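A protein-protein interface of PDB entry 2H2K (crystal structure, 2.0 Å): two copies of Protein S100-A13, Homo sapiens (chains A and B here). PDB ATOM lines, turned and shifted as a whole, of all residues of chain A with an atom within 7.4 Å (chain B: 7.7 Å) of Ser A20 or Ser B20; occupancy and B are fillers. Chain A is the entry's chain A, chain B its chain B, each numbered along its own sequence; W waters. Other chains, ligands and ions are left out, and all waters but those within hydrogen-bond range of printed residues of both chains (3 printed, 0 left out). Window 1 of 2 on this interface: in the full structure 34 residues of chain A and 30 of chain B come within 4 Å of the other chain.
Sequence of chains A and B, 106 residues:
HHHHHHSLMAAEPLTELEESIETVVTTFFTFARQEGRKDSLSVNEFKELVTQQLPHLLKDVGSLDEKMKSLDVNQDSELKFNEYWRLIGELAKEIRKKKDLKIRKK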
ATOM      1  N   LEU A  14      -2.543  -3.500 -23.856  1.00  0.00           N
ATOM      2  CA  LEU A  14      -3.355  -4.696 -23.678  1.00  0.00           C
ATOM      3  C   LEU A  14      -4.814  -4.327 -23.589  1.00  0.00           C
ATOM      4  O   LEU A  14      -5.161  -3.250 -23.104  1.00  0.00           O
ATOM      5  CB  LEU A  14      -2.959  -5.438 -22.404  1.00  0.00           C
ATOM      6  CG  LEU A  14      -1.651  -6.215 -22.498  1.00  0.00           C
ATOM      7  CD1 LEU A  14      -1.502  -7.109 -21.273  1.00  0.00           C
ATOM      8  CD2 LEU A  14      -1.651  -7.054 -23.771  1.00  0.00           C
ATOM      9  N   THR A  15      -5.679  -5.205 -24.080  1.00  0.00           N
ATOM     10  CA  THR A  15      -7.087  -4.909 -23.986  1.00  0.00           C
ATOM     11  C   THR A  15      -7.420  -5.061 -22.526  1.00  0.00           C
ATOM     12  O   THR A  15      -6.613  -5.535 -21.721  1.00  0.00           O
ATOM     13  CB  THR A  15      -7.970  -5.888 -24.777  1.00  0.00           C
ATOM     14  OG1 THR A  15      -7.760  -7.223 -24.298  1.00  0.00           O
ATOM     15  CG2 THR A  15      -7.655  -5.805 -26.257  1.00  0.00           C
ATOM     16  N   GLU A  16      -8.625  -4.653 -22.197  1.00  0.00           N
ATOM     17  CA  GLU A  16      -9.105  -4.722 -20.847  1.00  0.00           C
ATOM     18  C   GLU A  16      -9.167  -6.180 -20.369  1.00  0.00           C
ATOM     19  O   GLU A  16      -8.867  -6.466 -19.213  1.00  0.00           O
ATOM     20  CB  GLU A  16     -10.456  -4.015 -20.808  1.00  0.00           C
ATOM     21  CG  GLU A  16     -10.421  -2.684 -21.599  1.00  0.00           C
ATOM     22  CD  GLU A  16     -10.520  -2.867 -23.121  1.00  0.00           C
ATOM     23  OE1 GLU A  16     -11.653  -3.006 -23.622  1.00  0.00           O
ATOM     24  OE2 GLU A  16      -9.481  -2.878 -23.820  1.00  0.00           O
ATOM     25  N   LEU A  17      -9.518  -7.101 -21.266  1.00  0.00           N
ATOM     26  CA  LEU A  17      -9.589  -8.521 -20.909  1.00  0.00           C
ATOM     27  C   LEU A  17      -8.201  -9.139 -20.710  1.00  0.00           C
ATOM     28  O   LEU A  17      -7.963  -9.846 -19.728  1.00  0.00           O
ATOM     29  CB  LEU A  17     -10.326  -9.319 -21.988  1.00  0.00           C
ATOM     30  CG  LEU A  17     -10.351 -10.843 -21.767  1.00  0.00           C
ATOM     31  CD1 LEU A  17     -11.055 -11.152 -20.454  1.00  0.00           C
ATOM     32  CD2 LEU A  17     -11.070 -11.537 -22.921  1.00  0.00           C
ATOM     33  N   GLU A  18      -7.292  -8.879 -21.646  1.00  0.00           N
ATOM     34  CA  GLU A  18      -5.940  -9.426 -21.568  1.00  0.00           C
ATOM     35  C   GLU A  18      -5.220  -8.942 -20.311  1.00  0.00           C
ATOM     36  O   GLU A  18      -4.513  -9.702 -19.651  1.00  0.00           O
ATOM     37  CB  GLU A  18      -5.139  -9.026 -22.814  1.00  0.00           C
ATOM     38  CG  GLU A  18      -5.738  -9.535 -24.120  1.00  0.00           C
ATOM     39  CD  GLU A  18      -5.017  -8.998 -25.347  1.00  0.00           C
ATOM     40  OE1 GLU A  18      -4.638  -7.812 -25.331  1.00  0.00           O
ATOM     41  OE2 GLU A  18      -4.845  -9.755 -26.325  1.00  0.00           O
ATOM     42  N   GLU A  19      -5.416  -7.672 -19.982  1.00  0.00           N
ATOM     43  CA  GLU A  19      -4.796  -7.076 -18.809  1.00  0.00           C
ATOM     44  C   GLU A  19      -5.349  -7.710 -17.524  1.00  0.00           C
ATOM     45  O   GLU A  19      -4.614  -7.913 -16.553  1.00  0.00           O
ATOM     46  CB  GLU A  19      -5.045  -5.571 -18.828  1.00  0.00           C
ATOM     47  CG  GLU A  19      -4.279  -4.769 -17.804  1.00  0.00           C
ATOM     48  CD  GLU A  19      -4.422  -3.281 -18.048  1.00  0.00           C
ATOM     49  OE1 GLU A  19      -5.483  -2.871 -18.562  1.00  0.00           O
ATOM     50  OE2 GLU A  19      -3.488  -2.519 -17.719  1.00  0.00           O
ATOM     51  N   SER A  20      -6.642  -8.027 -17.529  1.00  0.00           N
ATOM     52  CA  SER A  20      -7.281  -8.650 -16.375  1.00  0.00           C
ATOM     53  C   SER A  20      -6.753 -10.066 -16.165  1.00  0.00           C
ATOM     54  O   SER A  20      -6.504 -10.494 -15.042  1.00  0.00           O
ATOM     55  CB  SER A  20      -8.797  -8.687 -16.570  1.00  0.00           C
ATOM     56  OG  SER A  20      -9.344  -7.386 -16.522  1.00  0.00           O
ATOM     57  N   ILE A  21      -6.590 -10.804 -17.256  1.00  0.00           N
ATOM     58  CA  ILE A  21      -6.072 -12.155 -17.151  1.00  0.00           C
ATOM     59  C   ILE A  21      -4.649 -12.096 -16.614  1.00  0.00           C
ATOM     60  O   ILE A  21      -4.292 -12.822 -15.684  1.00  0.00           O
ATOM     61  CB  ILE A  21      -6.058 -12.866 -18.517  1.00  0.00           C
ATOM     62  CG1 ILE A  21      -7.481 -12.957 -19.070  1.00  0.00           C
ATOM     63  CG2 ILE A  21      -5.470 -14.262 -18.357  1.00  0.00           C
ATOM     64  CD1 ILE A  21      -7.531 -13.384 -20.526  1.00  0.00           C
ATOM     65  N   GLU A  22      -3.833 -11.218 -17.188  1.00  0.00           N
ATOM     66  CA  GLU A  22      -2.456 -11.120 -16.738  1.00  0.00           C
ATOM     67  C   GLU A  22      -2.370 -10.740 -15.259  1.00  0.00           C
ATOM     68  O   GLU A  22      -1.508 -11.237 -14.537  1.00  0.00           O
ATOM     69  CB  GLU A  22      -1.670 -10.135 -17.626  1.00  0.00           C
ATOM     70  CG  GLU A  22      -1.366  -8.772 -17.027  1.00  0.00           C
ATOM     71  CD  GLU A  22      -0.153  -8.117 -17.684  1.00  0.00           C
ATOM     72  OE1 GLU A  22       0.679  -8.854 -18.259  1.00  0.00           O
ATOM     73  OE2 GLU A  22      -0.020  -6.877 -17.616  1.00  0.00           O
ATOM     74  N   THR A  23      -3.272  -9.878 -14.804  1.00  0.00           N
ATOM     75  CA  THR A  23      -3.284  -9.466 -13.402  1.00  0.00           C
ATOM     76  C   THR A  23      -3.591 -10.638 -12.469  1.00  0.00           C
ATOM     77  O   THR A  23      -2.997 -10.766 -11.401  1.00  0.00           O
ATOM     78  CB  THR A  23      -4.318  -8.350 -13.160  1.00  0.00           C
ATOM     79  OG1 THR A  23      -3.870  -7.154 -13.799  1.00  0.00           O
ATOM     80  CG2 THR A  23      -4.500  -8.091 -11.659  1.00  0.00           C
ATOM     81  N   VAL A  24      -4.524 -11.494 -12.870  1.00  0.00           N
ATOM     82  CA  VAL A  24      -4.865 -12.655 -12.053  1.00  0.00           C
ATOM     83  C   VAL A  24      -3.628 -13.523 -11.841  1.00  0.00           C
ATOM     84  O   VAL A  24      -3.376 -14.037 -10.738  1.00  0.00           O
ATOM     85  CB  VAL A  24      -5.952 -13.515 -12.722  1.00  0.00           C
ATOM     86  CG1 VAL A  24      -6.213 -14.778 -11.884  1.00  0.00           C
ATOM     87  CG2 VAL A  24      -7.222 -12.705 -12.867  1.00  0.00           C
ATOM     88  N   VAL A  25      -2.848 -13.674 -12.905  1.00  0.00           N
ATOM     89  CA  VAL A  25      -1.641 -14.490 -12.852  1.00  0.00           C
ATOM     90  C   VAL A  25      -0.521 -13.823 -12.049  1.00  0.00           C
ATOM     91  O   VAL A  25       0.104 -14.462 -11.206  1.00  0.00           O
ATOM     92  CB  VAL A  25      -1.142 -14.819 -14.277  1.00  0.00           C
ATOM     93  CG1 VAL A  25       0.117 -15.674 -14.214  1.00  0.00           C
ATOM     94  CG2 VAL A  25      -2.238 -15.562 -15.049  1.00  0.00           C
ATOM     95  N   THR A  26      -0.274 -12.540 -12.292  1.00  0.00           N
ATOM     96  CA  THR A  26       0.788 -11.847 -11.579  1.00  0.00           C
ATOM     97  C   THR A  26       0.532 -11.803 -10.077  1.00  0.00           C
ATOM     98  O   THR A  26       1.455 -11.947  -9.280  1.00  0.00           O
ATOM     99  CB  THR A  26       0.978 -10.412 -12.097  1.00  0.00           C
ATOM    100  OG1 THR A  26      -0.239  -9.677 -11.942  1.00  0.00           O
ATOM    101  CG2 THR A  26       1.364 -10.425 -13.564  1.00  0.00           C
ATOM    102  N   THR A  27      -0.723 -11.605  -9.691  1.00  0.00           N
ATOM    103  CA  THR A  27      -1.078 -11.562  -8.279  1.00  0.00           C
ATOM    104  C   THR A  27      -0.617 -12.841  -7.576  1.00  0.00           C
ATOM    105  O   THR A  27      -0.082 -12.786  -6.468  1.00  0.00           O
ATOM    106  CB  THR A  27      -2.600 -11.389  -8.105  1.00  0.00           C
ATOM    107  OG1 THR A  27      -2.996 -10.135  -8.679  1.00  0.00           O
ATOM    108  CG2 THR A  27      -2.978 -11.413  -6.632  1.00  0.00           C
ATOM    109  N   TRP A  85      -5.799 -21.359  -9.486  1.00  0.00           N
ATOM    110  CA  TRP A  85      -6.688 -21.135 -10.616  1.00  0.00           C
ATOM    111  C   TRP A  85      -8.087 -21.696 -10.356  1.00  0.00           C
ATOM    112  O   TRP A  85      -9.077 -21.098 -10.770  1.00  0.00           O
ATOM    113  CB  TRP A  85      -6.117 -21.743 -11.897  1.00  0.00           C
ATOM    114  CG  TRP A  85      -6.932 -21.359 -13.104  1.00  0.00           C
ATOM    115  CD1 TRP A  85      -7.746 -22.171 -13.848  1.00  0.00           C
ATOM    116  CD2 TRP A  85      -7.084 -20.037 -13.640  1.00  0.00           C
ATOM    117  NE1 TRP A  85      -8.398 -21.431 -14.813  1.00  0.00           N
ATOM    118  CE2 TRP A  85      -8.011 -20.121 -14.705  1.00  0.00           C
ATOM    119  CE3 TRP A  85      -6.525 -18.788 -13.320  1.00  0.00           C
ATOM    120  CZ2 TRP A  85      -8.396 -18.997 -15.453  1.00  0.00           C
ATOM    121  CZ3 TRP A  85      -6.907 -17.672 -14.068  1.00  0.00           C
ATOM    122  CH2 TRP A  85      -7.835 -17.787 -15.122  1.00  0.00           C
ATOM    123  N   ILE A  88      -9.980 -19.163  -8.465  1.00  0.00           N
ATOM    124  CA  ILE A  88     -10.424 -18.059  -9.296  1.00  0.00           C
ATOM    125  C   ILE A  88     -11.680 -18.471 -10.066  1.00  0.00           C
ATOM    126  O   ILE A  88     -12.595 -17.671 -10.263  1.00  0.00           O
ATOM    127  CB  ILE A  88      -9.342 -17.669 -10.293  1.00  0.00           C
ATOM    128  CG1 ILE A  88      -8.041 -17.367  -9.551  1.00  0.00           C
ATOM    129  CG2 ILE A  88      -9.793 -16.445 -11.096  1.00  0.00           C
ATOM    130  CD1 ILE A  88      -7.990 -15.988  -8.967  1.00  0.00           C
ATOM    131  N   ILE A  95     -19.572 -14.832  -9.461  1.00  0.00           N
ATOM    132  CA  ILE A  95     -19.803 -13.549 -10.120  1.00  0.00           C
ATOM    133  C   ILE A  95     -20.813 -13.745 -11.258  1.00  0.00           C
ATOM    134  O   ILE A  95     -21.752 -12.962 -11.403  1.00  0.00           O
ATOM    135  CB  ILE A  95     -18.479 -12.966 -10.694  1.00  0.00           C
ATOM    136  CG1 ILE A  95     -17.591 -12.455  -9.556  1.00  0.00           C
ATOM    137  CG2 ILE A  95     -18.764 -11.873 -11.707  1.00  0.00           C
ATOM    138  CD1 ILE A  95     -16.396 -11.649 -10.028  1.00  0.00           C
ATOM    139  N   LEU B  14     -13.793  -2.619  -4.830  1.00  0.00           N
ATOM    140  CA  LEU B  14     -13.110  -3.850  -5.204  1.00  0.00           C
ATOM    141  C   LEU B  14     -11.598  -3.647  -5.260  1.00  0.00           C
ATOM    142  O   LEU B  14     -11.120  -2.533  -5.469  1.00  0.00           O
ATOM    143  CB  LEU B  14     -13.622  -4.361  -6.551  1.00  0.00           C
ATOM    144  CG  LEU B  14     -15.114  -4.695  -6.627  1.00  0.00           C
ATOM    145  CD1 LEU B  14     -15.449  -5.361  -7.953  1.00  0.00           C
ATOM    146  CD2 LEU B  14     -15.526  -5.577  -5.459  1.00  0.00           C
ATOM    147  N   THR B  15     -10.854  -4.732  -5.072  1.00  0.00           N
ATOM    148  CA  THR B  15      -9.414  -4.700  -5.217  1.00  0.00           C
ATOM    149  C   THR B  15      -9.090  -4.931  -6.687  1.00  0.00           C
ATOM    150  O   THR B  15      -9.953  -5.294  -7.484  1.00  0.00           O
ATOM    151  CB  THR B  15      -8.743  -5.817  -4.416  1.00  0.00           C
ATOM    152  OG1 THR B  15      -9.168  -7.085  -4.934  1.00  0.00           O
ATOM    153  CG2 THR B  15      -9.119  -5.718  -2.940  1.00  0.00           C
ATOM    154  N   GLU B  16      -7.831  -4.729  -7.028  1.00  0.00           N
ATOM    155  CA  GLU B  16      -7.363  -4.918  -8.384  1.00  0.00           C
ATOM    156  C   GLU B  16      -7.660  -6.344  -8.865  1.00  0.00           C
ATOM    157  O   GLU B  16      -8.125  -6.548  -9.986  1.00  0.00           O
ATOM    158  CB  GLU B  16      -5.863  -4.641  -8.430  1.00  0.00           C
ATOM    159  CG  GLU B  16      -5.308  -4.434  -9.806  1.00  0.00           C
ATOM    160  CD  GLU B  16      -4.120  -3.495  -9.800  1.00  0.00           C
ATOM    161  OE1 GLU B  16      -3.836  -2.902  -8.735  1.00  0.00           O
ATOM    162  OE2 GLU B  16      -3.479  -3.347 -10.861  1.00  0.00           O
ATOM    163  N   LEU B  17      -7.394  -7.331  -8.015  1.00  0.00           N
ATOM    164  CA  LEU B  17      -7.645  -8.718  -8.389  1.00  0.00           C
ATOM    165  C   LEU B  17      -9.135  -8.975  -8.608  1.00  0.00           C
ATOM    166  O   LEU B  17      -9.525  -9.589  -9.604  1.00  0.00           O
ATOM    167  CB  LEU B  17      -7.116  -9.673  -7.317  1.00  0.00           C
ATOM    168  CG  LEU B  17      -7.385 -11.152  -7.615  1.00  0.00           C
ATOM    169  CD1 LEU B  17      -6.730 -11.523  -8.928  1.00  0.00           C
ATOM    170  CD2 LEU B  17      -6.855 -12.036  -6.473  1.00  0.00           C
ATOM    171  N   GLU B  18      -9.970  -8.504  -7.684  1.00  0.00           N
ATOM    172  CA  GLU B  18     -11.409  -8.719  -7.801  1.00  0.00           C
ATOM    173  C   GLU B  18     -11.999  -8.077  -9.054  1.00  0.00           C
ATOM    174  O   GLU B  18     -12.860  -8.667  -9.704  1.00  0.00           O
ATOM    175  CB  GLU B  18     -12.121  -8.202  -6.547  1.00  0.00           C
ATOM    176  CG  GLU B  18     -11.646  -8.888  -5.277  1.00  0.00           C
ATOM    177  CD  GLU B  18     -12.266  -8.306  -4.026  1.00  0.00           C
ATOM    178  OE1 GLU B  18     -12.425  -7.069  -3.973  1.00  0.00           O
ATOM    179  OE2 GLU B  18     -12.567  -9.077  -3.090  1.00  0.00           O
ATOM    180  N   GLU B  19     -11.543  -6.871  -9.393  1.00  0.00           N
ATOM    181  CA  GLU B  19     -12.047  -6.195 -10.586  1.00  0.00           C
ATOM    182  C   GLU B  19     -11.604  -6.949 -11.844  1.00  0.00           C
ATOM    183  O   GLU B  19     -12.353  -7.039 -12.818  1.00  0.00           O
ATOM    184  CB  GLU B  19     -11.542  -4.750 -10.664  1.00  0.00           C
ATOM    185  CG  GLU B  19     -11.938  -3.866  -9.485  1.00  0.00           C
ATOM    186  CD  GLU B  19     -11.872  -2.382  -9.813  1.00  0.00           C
ATOM    187  OE1 GLU B  19     -10.886  -1.955 -10.451  1.00  0.00           O
ATOM    188  OE2 GLU B  19     -12.803  -1.645  -9.425  1.00  0.00           O
ATOM    189  N   SER B  20     -10.386  -7.481 -11.824  1.00  0.00           N
ATOM    190  CA  SER B  20      -9.875  -8.229 -12.964  1.00  0.00           C
ATOM    191  C   SER B  20     -10.731  -9.470 -13.187  1.00  0.00           C
ATOM    192  O   SER B  20     -11.113  -9.768 -14.319  1.00  0.00           O
ATOM    193  CB  SER B  20      -8.417  -8.630 -12.732  1.00  0.00           C
ATOM    194  OG  SER B  20      -7.574  -7.490 -12.682  1.00  0.00           O
ATOM    195  N   ILE B  21     -11.038 -10.194 -12.114  1.00  0.00           N
ATOM    196  CA  ILE B  21     -11.877 -11.385 -12.265  1.00  0.00           C
ATOM    197  C   ILE B  21     -13.248 -10.986 -12.801  1.00  0.00           C
ATOM    198  O   ILE B  21     -13.790 -11.649 -13.689  1.00  0.00           O
ATOM    199  CB  ILE B  21     -12.074 -12.128 -10.925  1.00  0.00           C
ATOM    200  CG1 ILE B  21     -10.713 -12.533 -10.352  1.00  0.00           C
ATOM    201  CG2 ILE B  21     -12.972 -13.355 -11.119  1.00  0.00           C
ATOM    202  CD1 ILE B  21     -10.780 -13.160  -8.979  1.00  0.00           C
ATOM    203  N   GLU B  22     -13.799  -9.886 -12.286  1.00  0.00           N
ATOM    204  CA  GLU B  22     -15.105  -9.424 -12.751  1.00  0.00           C
ATOM    205  C   GLU B  22     -15.095  -9.055 -14.237  1.00  0.00           C
ATOM    206  O   GLU B  22     -16.063  -9.320 -14.948  1.00  0.00           O
ATOM    207  CB  GLU B  22     -15.591  -8.221 -11.930  1.00  0.00           C
ATOM    208  CG  GLU B  22     -16.784  -7.518 -12.561  1.00  0.00           C
ATOM    209  CD  GLU B  22     -17.586  -6.673 -11.591  1.00  0.00           C
ATOM    210  OE1 GLU B  22     -17.124  -6.447 -10.453  1.00  0.00           O
ATOM    211  OE2 GLU B  22     -18.686  -6.227 -11.980  1.00  0.00           O
ATOM    212  N   THR B  23     -14.013  -8.435 -14.699  1.00  0.00           N
ATOM    213  CA  THR B  23     -13.908  -8.065 -16.108  1.00  0.00           C
ATOM    214  C   THR B  23     -13.921  -9.309 -17.006  1.00  0.00           C
ATOM    215  O   THR B  23     -14.534  -9.312 -18.066  1.00  0.00           O
ATOM    216  CB  THR B  23     -12.612  -7.268 -16.375  1.00  0.00           C
ATOM    217  OG1 THR B  23     -12.669  -6.021 -15.677  1.00  0.00           O
ATOM    218  CG2 THR B  23     -12.438  -7.000 -17.860  1.00  0.00           C
ATOM    219  N   VAL B  24     -13.238 -10.367 -16.584  1.00  0.00           N
ATOM    220  CA  VAL B  24     -13.216 -11.583 -17.397  1.00  0.00           C
ATOM    221  C   VAL B  24     -14.630 -12.142 -17.557  1.00  0.00           C
ATOM    222  O   VAL B  24     -14.998 -12.633 -18.624  1.00  0.00           O
ATOM    223  CB  VAL B  24     -12.320 -12.667 -16.780  1.00  0.00           C
ATOM    224  CG1 VAL B  24     -12.411 -13.953 -17.611  1.00  0.00           C
ATOM    225  CG2 VAL B  24     -10.888 -12.171 -16.728  1.00  0.00           C
ATOM    226  N   VAL B  25     -15.428 -12.059 -16.496  1.00  0.00           N
ATOM    227  CA  VAL B  25     -16.795 -12.566 -16.549  1.00  0.00           C
ATOM    228  C   VAL B  25     -17.704 -11.652 -17.366  1.00  0.00           C
ATOM    229  O   VAL B  25     -18.483 -12.124 -18.191  1.00  0.00           O
ATOM    230  CB  VAL B  25     -17.406 -12.723 -15.132  1.00  0.00           C
ATOM    231  CG1 VAL B  25     -18.850 -13.172 -15.236  1.00  0.00           C
ATOM    232  CG2 VAL B  25     -16.608 -13.720 -14.315  1.00  0.00           C
ATOM    233  N   THR B  26     -17.601 -10.345 -17.154  1.00  0.00           N
ATOM    234  CA  THR B  26     -18.455  -9.413 -17.880  1.00  0.00           C
ATOM    235  C   THR B  26     -18.156  -9.367 -19.374  1.00  0.00           C
ATOM    236  O   THR B  26     -19.054  -9.126 -20.177  1.00  0.00           O
ATOM    237  CB  THR B  26     -18.366  -7.974 -17.305  1.00  0.00           C
ATOM    238  OG1 THR B  26     -17.031  -7.476 -17.440  1.00  0.00           O
ATOM    239  CG2 THR B  26     -18.747  -7.965 -15.837  1.00  0.00           C
ATOM    240  N   THR B  27     -16.905  -9.606 -19.754  1.00  0.00           N
ATOM    241  CA  THR B  27     -16.545  -9.587 -21.169  1.00  0.00           C
ATOM    242  C   THR B  27     -17.315 -10.679 -21.907  1.00  0.00           C
ATOM    243  O   THR B  27     -17.804 -10.464 -23.020  1.00  0.00           O
ATOM    244  CB  THR B  27     -15.026  -9.787 -21.370  1.00  0.00           C
ATOM    245  OG1 THR B  27     -14.323  -8.732 -20.699  1.00  0.00           O
ATOM    246  CG2 THR B  27     -14.670  -9.752 -22.856  1.00  0.00           C
ATOM    247  N   GLN B  53     -10.849  -8.392 -28.276  1.00  0.00           N
ATOM    248  CA  GLN B  53     -10.495  -8.349 -26.863  1.00  0.00           C
ATOM    249  C   GLN B  53      -9.316  -9.268 -26.561  1.00  0.00           C
ATOM    250  O   GLN B  53      -8.793  -9.277 -25.447  1.00  0.00           O
ATOM    251  CB  GLN B  53     -11.696  -8.733 -25.996  1.00  0.00           C
ATOM    252  CG  GLN B  53     -12.570  -7.558 -25.589  1.00  0.00           C
ATOM    253  CD  GLN B  53     -11.787  -6.466 -24.887  1.00  0.00           C
ATOM    254  OE1 GLN B  53     -11.806  -5.311 -25.312  1.00  0.00           O
ATOM    255  NE2 GLN B  53     -11.097  -6.828 -23.812  1.00  0.00           N
ATOM    256  N   TRP B  85     -14.516 -20.242 -20.088  1.00  0.00           N
ATOM    257  CA  TRP B  85     -13.574 -20.247 -18.968  1.00  0.00           C
ATOM    258  C   TRP B  85     -12.360 -21.143 -19.244  1.00  0.00           C
ATOM    259  O   TRP B  85     -11.242 -20.829 -18.831  1.00  0.00           O
ATOM    260  CB  TRP B  85     -14.259 -20.705 -17.681  1.00  0.00           C
ATOM    261  CG  TRP B  85     -13.373 -20.492 -16.484  1.00  0.00           C
ATOM    262  CD1 TRP B  85     -12.700 -21.445 -15.772  1.00  0.00           C
ATOM    263  CD2 TRP B  85     -12.996 -19.227 -15.919  1.00  0.00           C
ATOM    264  NE1 TRP B  85     -11.928 -20.849 -14.799  1.00  0.00           N
ATOM    265  CE2 TRP B  85     -12.094 -19.494 -14.864  1.00  0.00           C
ATOM    266  CE3 TRP B  85     -13.342 -17.901 -16.199  1.00  0.00           C
ATOM    267  CZ2 TRP B  85     -11.518 -18.469 -14.093  1.00  0.00           C
ATOM    268  CZ3 TRP B  85     -12.774 -16.880 -15.434  1.00  0.00           C
ATOM    269  CH2 TRP B  85     -11.874 -17.173 -14.387  1.00  0.00           C
ATOM    270  N   ILE B  88      -9.940 -19.165 -21.081  1.00  0.00           N
ATOM    271  CA  ILE B  88      -9.233 -18.249 -20.195  1.00  0.00           C
ATOM    272  C   ILE B  88      -8.131 -18.981 -19.435  1.00  0.00           C
ATOM    273  O   ILE B  88      -7.029 -18.459 -19.264  1.00  0.00           O
ATOM    274  CB  ILE B  88     -10.194 -17.594 -19.175  1.00  0.00           C
ATOM    275  CG1 ILE B  88     -11.333 -16.875 -19.916  1.00  0.00           C
ATOM    276  CG2 ILE B  88      -9.419 -16.601 -18.299  1.00  0.00           C
ATOM    277  CD1 ILE B  88     -10.853 -15.757 -20.818  1.00  0.00           C
ATOM    278  N   ILE B  95       0.601 -17.344 -19.801  1.00  0.00           N
ATOM    279  CA  ILE B  95       1.144 -16.161 -19.146  1.00  0.00           C
ATOM    280  C   ILE B  95       1.934 -16.612 -17.925  1.00  0.00           C
ATOM    281  O   ILE B  95       2.990 -16.059 -17.617  1.00  0.00           O
ATOM    282  CB  ILE B  95       0.020 -15.216 -18.694  1.00  0.00           C
ATOM    283  CG1 ILE B  95      -0.679 -14.625 -19.920  1.00  0.00           C
ATOM    284  CG2 ILE B  95       0.577 -14.118 -17.800  1.00  0.00           C
ATOM    285  CD1 ILE B  95      -1.962 -13.891 -19.579  1.00  0.00           C
HETATM  286  O   HOH W   1     -10.952 -22.453 -12.666  1.00  0.00           O
HETATM  287  O   HOH W   2      -8.564  -5.598 -14.754  1.00  0.00           O
HETATM  288  O   HOH W   3      -9.968 -22.584 -16.904  1.00  0.00           O
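N of Leu A17 sits close to NE2 of Gln B53 (3.0 Å).
O of Gln B53 lies within hydrogen-bond range of OG1 of Thr A15, at 2.6 Å.
The side-chain carboxylate (OE1) of Glu A16 sits close to the side-chain amide oxygen (OE1) of Gln B53 (2.9 Å).
Water W2 bridges OG of Ser A20 (2.6 Å) and OG of Ser B20 (3.0 Å).
Water W1 lies within hydrogen-bond range of NE1 of Trp B85 (2.8 Å) and O of Trp A85 (3.0 Å).
Water W3 lies within hydrogen-bond range of NE1 of Trp A85 (2.9 Å) and O of Trp B85 (2.9 Å).
Of the 17 printed residues of chain A, 14 touch a printed residue of chain B.
Hydrophobic or aromatic side chains of chain A that line the printed part of chain B: Leu A17, Ile A21, Val A25, Trp A85, Ile A88 and Ile A95.
Printed residues of chain B that touch a printed residue of chain A: Leu B17, Ser B20, Ile B21, Glu B22, Thr B23, Val B24, Val B25, Gln B53, Trp B85, Ile B88 and Ile B95.
Hydrophobic or aromatic side chains of chain B within 4 Å of the printed part of chain A: Leu B17, Ile B21, Val B24, Val B25, Trp B85, Ile B88 and Ile B95.
Among the printed residues, no Asp or Glu carboxylate lies within 4 Å of a Lys or Arg side-chain nitrogen of the other chain.
Among the printed residues, merely in contact across the chains: Ser A20 with Thr B23 (3.3 Å), Thr A23 with Ser B20 (3.3 Å), Glu A18 with Gln B53 (3.3 Å), Ser A20 with Ser B20 (3.4 Å), Trp A85 with Trp B85 (3.4 Å), Ile A21 with Ile B95 (3.7 Å), Trp A85 with Ile B88 (3.7 Å), Ile A95 with Glu B22 (3.7 Å), Ile A95 with Val B25 (3.8 Å), Leu A17 with Val B24 (3.8 Å), Val A24 with Leu B17 (3.8 Å), Glu A16 with Thr B23 (3.9 Å), Thr A27 with Leu B17 (3.9 Å), Val A25 with Ile B95 (3.9 Å), Ile A88 with Trp B85 (3.96 Å), Ile A88 with Ile B21 (3.97 Å), Ile A95 with Ile B21 (3.98 Å) and Glu A22 with Ile B95 (3.999 Å).
The side-chain hydroxyl of Thr A26 sits at hydrogen-bond distance from the backbone carbonyl oxygen of Thr A23, at 3.0 Å.
The backbone carbonyl oxygen (O) of Glu A22 sits close to the side-chain hydroxyl (OG1) of Thr A26 (3.3 Å).
The backbone carbonyl oxygen of Thr B23 lies within hydrogen-bond range of the side-chain hydroxyl of Thr B27.
OG of Ser B20 sits at hydrogen-bond distance from O of Glu B16 (2.9 Å).
OG1 of Thr B23 is in hydrogen-bond range of O of Glu B19.
OG1 of Thr A27 is in hydrogen-bond range of O of Thr A23.
Ser B20 touches its own counterpart, Ser A20.
Ile A21 touches Ile B95, and with the chains exchanged Ile A95 touches Ile B21.
Thr A27 touches Leu B17, but with the chains exchanged Leu A17 does not touch Thr B27 (4.02 Å).
Trp A85 touches its own counterpart, Trp B85.
Positions printed for both chains: 14, 15, 16, 17, 18, 19, 20, 21, 22, 23, 24, 25, 26, 27, 85, 88 and 95.
Of the 21 pairs that touch across the chains among the printed residues, 14 have their exchanged pair printed and touching as well.
Ser A20 touches just these residues of chain B: Ser B20 (3.4 Å) and Thr B23 (3.3 Å).
Of the printed residues of chain B, Leu A17 touches Val B24 (3.8 Å) and Gln B53 (3.0 Å).
Printed residues of chain B within 4 Å of Ile A95: Ile B21, Glu B22 and Val B25.
Of the printed residues of chain B, Val A25 touches Ile B95 (3.9 Å).
Leu A14 touches none of the printed residues of chain B.
Thr B15 touches none of the printed residues of chain A.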
